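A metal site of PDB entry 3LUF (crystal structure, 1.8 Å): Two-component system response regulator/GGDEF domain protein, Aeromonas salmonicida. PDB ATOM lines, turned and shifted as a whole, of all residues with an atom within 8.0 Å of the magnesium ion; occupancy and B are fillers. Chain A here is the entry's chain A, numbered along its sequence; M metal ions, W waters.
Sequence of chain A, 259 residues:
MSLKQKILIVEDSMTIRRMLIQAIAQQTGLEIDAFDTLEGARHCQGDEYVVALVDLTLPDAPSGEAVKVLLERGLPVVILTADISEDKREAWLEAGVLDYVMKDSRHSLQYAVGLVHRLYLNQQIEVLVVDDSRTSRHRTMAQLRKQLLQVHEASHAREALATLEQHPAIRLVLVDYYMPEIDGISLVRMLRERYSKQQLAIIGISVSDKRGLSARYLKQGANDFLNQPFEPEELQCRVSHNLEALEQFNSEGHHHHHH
The backbone NH of Asp 176 sits at hydrogen-bond distance from the backbone carbonyl oxygen of Val 130 (3.0 Å).
The magnesium ion is bound by the side-chain carboxylate (OD1) of Asp 132 (2.0 Å), water W1 (2.0 Å), the side-chain carboxylate (OD2) of Asp 176 (2.0 Å), water W3 (2.0 Å), water W2 (2.1 Å) and the backbone carbonyl oxygen (O) of Tyr 178 (2.1 Å).
The magnesium ion has six donor atoms within binding distance.
Water W1 bridges the side-chain carboxylate (OD1) of Asp 176 (2.7 Å) and the backbone NH (N) of Tyr 178 (3.2 Å).
Water W2 bridges OD1 of Asp 131 (2.7 Å) and OD1 of Asp 176 (3.4 Å).
Within 4 Å of the magnesium ion: Asp 132, Asp 176 and Tyr 178.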
ATOM      1  N   VAL A 130      12.952  22.976  10.233  1.00  0.00           N
ATOM      2  CA  VAL A 130      13.319  24.342  10.611  1.00  0.00           C
ATOM      3  C   VAL A 130      12.116  25.057  11.194  1.00  0.00           C
ATOM      4  O   VAL A 130      11.121  25.269  10.513  1.00  0.00           O
ATOM      5  CB  VAL A 130      13.868  25.149   9.409  1.00  0.00           C
ATOM      6  CG1 VAL A 130      14.596  26.415   9.924  1.00  0.00           C
ATOM      7  CG2 VAL A 130      14.796  24.299   8.563  1.00  0.00           C
ATOM      8  N   ASP A 131      12.150  25.434  12.472  1.00  0.00           N
ATOM      9  CA  ASP A 131      10.987  25.994  13.106  1.00  0.00           C
ATOM     10  C   ASP A 131      11.478  26.660  14.385  1.00  0.00           C
ATOM     11  O   ASP A 131      12.205  26.044  15.183  1.00  0.00           O
ATOM     12  CB  ASP A 131       9.989  24.860  13.450  1.00  0.00           C
ATOM     13  CG  ASP A 131       8.660  25.355  13.998  1.00  0.00           C
ATOM     14  OD1 ASP A 131       8.509  26.513  14.477  1.00  0.00           O
ATOM     15  OD2 ASP A 131       7.698  24.549  13.950  1.00  0.00           O
ATOM     16  N   ASP A 132      11.072  27.914  14.571  1.00  0.00           N
ATOM     17  CA  ASP A 132      11.568  28.653  15.745  1.00  0.00           C
ATOM     18  C   ASP A 132      10.774  28.395  17.023  1.00  0.00           C
ATOM     19  O   ASP A 132      11.223  28.794  18.103  1.00  0.00           O
ATOM     20  CB  ASP A 132      11.530  30.146  15.460  1.00  0.00           C
ATOM     21  CG  ASP A 132      10.121  30.677  15.246  1.00  0.00           C
ATOM     22  OD1 ASP A 132       9.295  30.076  14.473  1.00  0.00           O
ATOM     23  OD2 ASP A 132       9.848  31.768  15.792  1.00  0.00           O
ATOM     24  N   SER A 133       9.615  27.718  16.918  1.00  0.00           N
ATOM     25  CA  SER A 133       8.838  27.317  18.096  1.00  0.00           C
ATOM     26  C   SER A 133       9.334  25.941  18.546  1.00  0.00           C
ATOM     27  O   SER A 133       9.165  24.938  17.832  1.00  0.00           O
ATOM     28  CB  SER A 133       7.336  27.294  17.776  1.00  0.00           C
ATOM     29  OG  SER A 133       6.603  26.498  18.699  1.00  0.00           O
ATOM     30  N   ARG A 134       9.904  25.864  19.741  1.00  0.00           N
ATOM     31  CA  ARG A 134      10.356  24.556  20.252  1.00  0.00           C
ATOM     32  C   ARG A 134       9.232  23.531  20.318  1.00  0.00           C
ATOM     33  O   ARG A 134       9.454  22.355  19.987  1.00  0.00           O
ATOM     34  CB  ARG A 134      11.046  24.739  21.641  1.00  0.00           C
ATOM     35  CG  ARG A 134      11.639  23.412  22.214  1.00  0.00           C
ATOM     36  CD  ARG A 134      12.380  23.657  23.533  1.00  0.00           C
ATOM     37  NE  ARG A 134      13.638  24.348  23.261  1.00  0.00           N
ATOM     38  CZ  ARG A 134      13.814  25.672  23.365  1.00  0.00           C
ATOM     39  NH1 ARG A 134      12.807  26.462  23.766  1.00  0.00           N
ATOM     40  NH2 ARG A 134      15.001  26.202  23.046  1.00  0.00           N
ATOM     41  N   SER A 136       6.323  23.379  18.395  1.00  0.00           N
ATOM     42  CA  SER A 136       5.984  22.912  17.057  1.00  0.00           C
ATOM     43  C   SER A 136       7.145  22.078  16.494  1.00  0.00           C
ATOM     44  O   SER A 136       6.922  21.019  15.880  1.00  0.00           O
ATOM     45  CB  SER A 136       5.594  24.100  16.174  1.00  0.00           C
ATOM     46  OG  SER A 136       4.247  24.429  16.470  1.00  0.00           O
ATOM     47  N   SER A 155      16.528  25.672  14.732  1.00  0.00           N
ATOM     48  CA  SER A 155      15.595  26.676  15.299  1.00  0.00           C
ATOM     49  C   SER A 155      15.548  27.998  14.561  1.00  0.00           C
ATOM     50  O   SER A 155      14.865  28.922  14.997  1.00  0.00           O
ATOM     51  CB  SER A 155      15.933  26.958  16.775  1.00  0.00           C
ATOM     52  OG  SER A 155      16.106  25.754  17.486  1.00  0.00           O
ATOM     53  N   VAL A 175       9.902  23.772   6.275  1.00  0.00           N
ATOM     54  CA  VAL A 175      10.265  25.163   6.608  1.00  0.00           C
ATOM     55  C   VAL A 175       9.092  25.921   7.210  1.00  0.00           C
ATOM     56  O   VAL A 175       8.052  26.086   6.581  1.00  0.00           O
ATOM     57  CB  VAL A 175      10.766  25.921   5.345  1.00  0.00           C
ATOM     58  CG1 VAL A 175      11.057  27.401   5.673  1.00  0.00           C
ATOM     59  CG2 VAL A 175      12.017  25.255   4.744  1.00  0.00           C
ATOM     60  N   ASP A 176       9.266  26.382   8.455  1.00  0.00           N
ATOM     61  CA  ASP A 176       8.272  27.213   9.127  1.00  0.00           C
ATOM     62  C   ASP A 176       8.197  28.624   8.538  1.00  0.00           C
ATOM     63  O   ASP A 176       9.200  29.152   8.071  1.00  0.00           O
ATOM     64  CB  ASP A 176       8.647  27.285  10.637  1.00  0.00           C
ATOM     65  CG  ASP A 176       7.706  28.144  11.424  1.00  0.00           C
ATOM     66  OD1 ASP A 176       6.460  27.999  11.330  1.00  0.00           O
ATOM     67  OD2 ASP A 176       8.254  28.970  12.179  1.00  0.00           O
ATOM     68  N   TYR A 177       7.018  29.235   8.575  1.00  0.00           N
ATOM     69  CA  TYR A 177       6.833  30.512   7.885  1.00  0.00           C
ATOM     70  C   TYR A 177       7.415  31.735   8.594  1.00  0.00           C
ATOM     71  O   TYR A 177       8.032  32.575   7.930  1.00  0.00           O
ATOM     72  CB  TYR A 177       5.358  30.726   7.532  1.00  0.00           C
ATOM     73  CG  TYR A 177       4.415  30.706   8.728  1.00  0.00           C
ATOM     74  CD1 TYR A 177       4.036  31.876   9.347  1.00  0.00           C
ATOM     75  CD2 TYR A 177       3.862  29.502   9.197  1.00  0.00           C
ATOM     76  CE1 TYR A 177       3.152  31.873  10.414  1.00  0.00           C
ATOM     77  CE2 TYR A 177       2.975  29.494  10.302  1.00  0.00           C
ATOM     78  CZ  TYR A 177       2.636  30.697  10.889  1.00  0.00           C
ATOM     79  OH  TYR A 177       1.753  30.746  11.964  1.00  0.00           O
ATOM     80  N   TYR A 178       7.194  31.892   9.897  1.00  0.00           N
ATOM     81  CA  TYR A 178       7.681  33.104  10.576  1.00  0.00           C
ATOM     82  C   TYR A 178       8.762  32.702  11.568  1.00  0.00           C
ATOM     83  O   TYR A 178       8.516  31.859  12.466  1.00  0.00           O
ATOM     84  CB  TYR A 178       6.531  33.821  11.332  1.00  0.00           C
ATOM     85  CG  TYR A 178       7.011  34.958  12.162  1.00  0.00           C
ATOM     86  CD1 TYR A 178       7.289  36.179  11.576  1.00  0.00           C
ATOM     87  CD2 TYR A 178       7.222  34.808  13.542  1.00  0.00           C
ATOM     88  CE1 TYR A 178       7.733  37.246  12.333  1.00  0.00           C
ATOM     89  CE2 TYR A 178       7.674  35.848  14.322  1.00  0.00           C
ATOM     90  CZ  TYR A 178       7.935  37.081  13.698  1.00  0.00           C
ATOM     91  OH  TYR A 178       8.393  38.118  14.457  1.00  0.00           O
ATOM     92  N   MET A 179       9.951  33.262  11.403  1.00  0.00           N
ATOM     93  CA  MET A 179      11.070  32.965  12.270  1.00  0.00           C
ATOM     94  C   MET A 179      11.864  34.271  12.366  1.00  0.00           C
ATOM     95  O   MET A 179      11.809  35.064  11.456  1.00  0.00           O
ATOM     96  CB  MET A 179      11.955  31.876  11.661  1.00  0.00           C
ATOM     97  CG  MET A 179      11.232  30.535  11.553  1.00  0.00           C
ATOM     98  SD  MET A 179      12.451  29.153  10.900  1.00  0.00           S
ATOM     99  CE  MET A 179      12.621  29.686   9.020  1.00  0.00           C
ATOM    100  N   PRO A 180      12.645  34.439  13.450  1.00  0.00           N
ATOM    101  CA  PRO A 180      13.482  35.630  13.565  1.00  0.00           C
ATOM    102  C   PRO A 180      14.527  35.744  12.470  1.00  0.00           C
ATOM    103  O   PRO A 180      15.164  34.750  12.073  1.00  0.00           O
ATOM    104  CB  PRO A 180      14.182  35.441  14.938  1.00  0.00           C
ATOM    105  CG  PRO A 180      13.306  34.472  15.715  1.00  0.00           C
ATOM    106  CD  PRO A 180      12.719  33.561  14.648  1.00  0.00           C
ATOM    107  N   GLY A 184      10.486  32.055   6.539  1.00  0.00           N
ATOM    108  CA  GLY A 184      10.500  30.825   5.751  1.00  0.00           C
ATOM    109  C   GLY A 184      10.600  31.088   4.272  1.00  0.00           C
ATOM    110  O   GLY A 184      11.331  30.392   3.593  1.00  0.00           O
ATOM    111  N   GLN A 228      -0.568  24.167   9.042  1.00  0.00           N
ATOM    112  CA  GLN A 228      -0.643  23.933  10.482  1.00  0.00           C
ATOM    113  C   GLN A 228      -1.987  24.390  11.017  1.00  0.00           C
ATOM    114  O   GLN A 228      -2.558  25.318  10.485  1.00  0.00           O
ATOM    115  CB  GLN A 228       0.485  24.678  11.219  1.00  0.00           C
ATOM    116  CG  GLN A 228       1.666  23.752  11.452  1.00  0.00           C
ATOM    117  CD  GLN A 228       2.843  24.410  12.104  1.00  0.00           C
ATOM    118  OE1 GLN A 228       3.058  25.619  11.959  1.00  0.00           O
ATOM    119  NE2 GLN A 228       3.638  23.619  12.815  1.00  0.00           N
HETATM  120 MG    MG M   1       7.586  30.315  13.537  1.00  0.00          MG
HETATM  121  O   HOH W   1       5.924  30.414  12.430  1.00  0.00           O
HETATM  122  O   HOH W   2       6.841  28.689  14.620  1.00  0.00           O
HETATM  123  O   HOH W   3       6.868  31.568  14.969  1.00  0.00           O
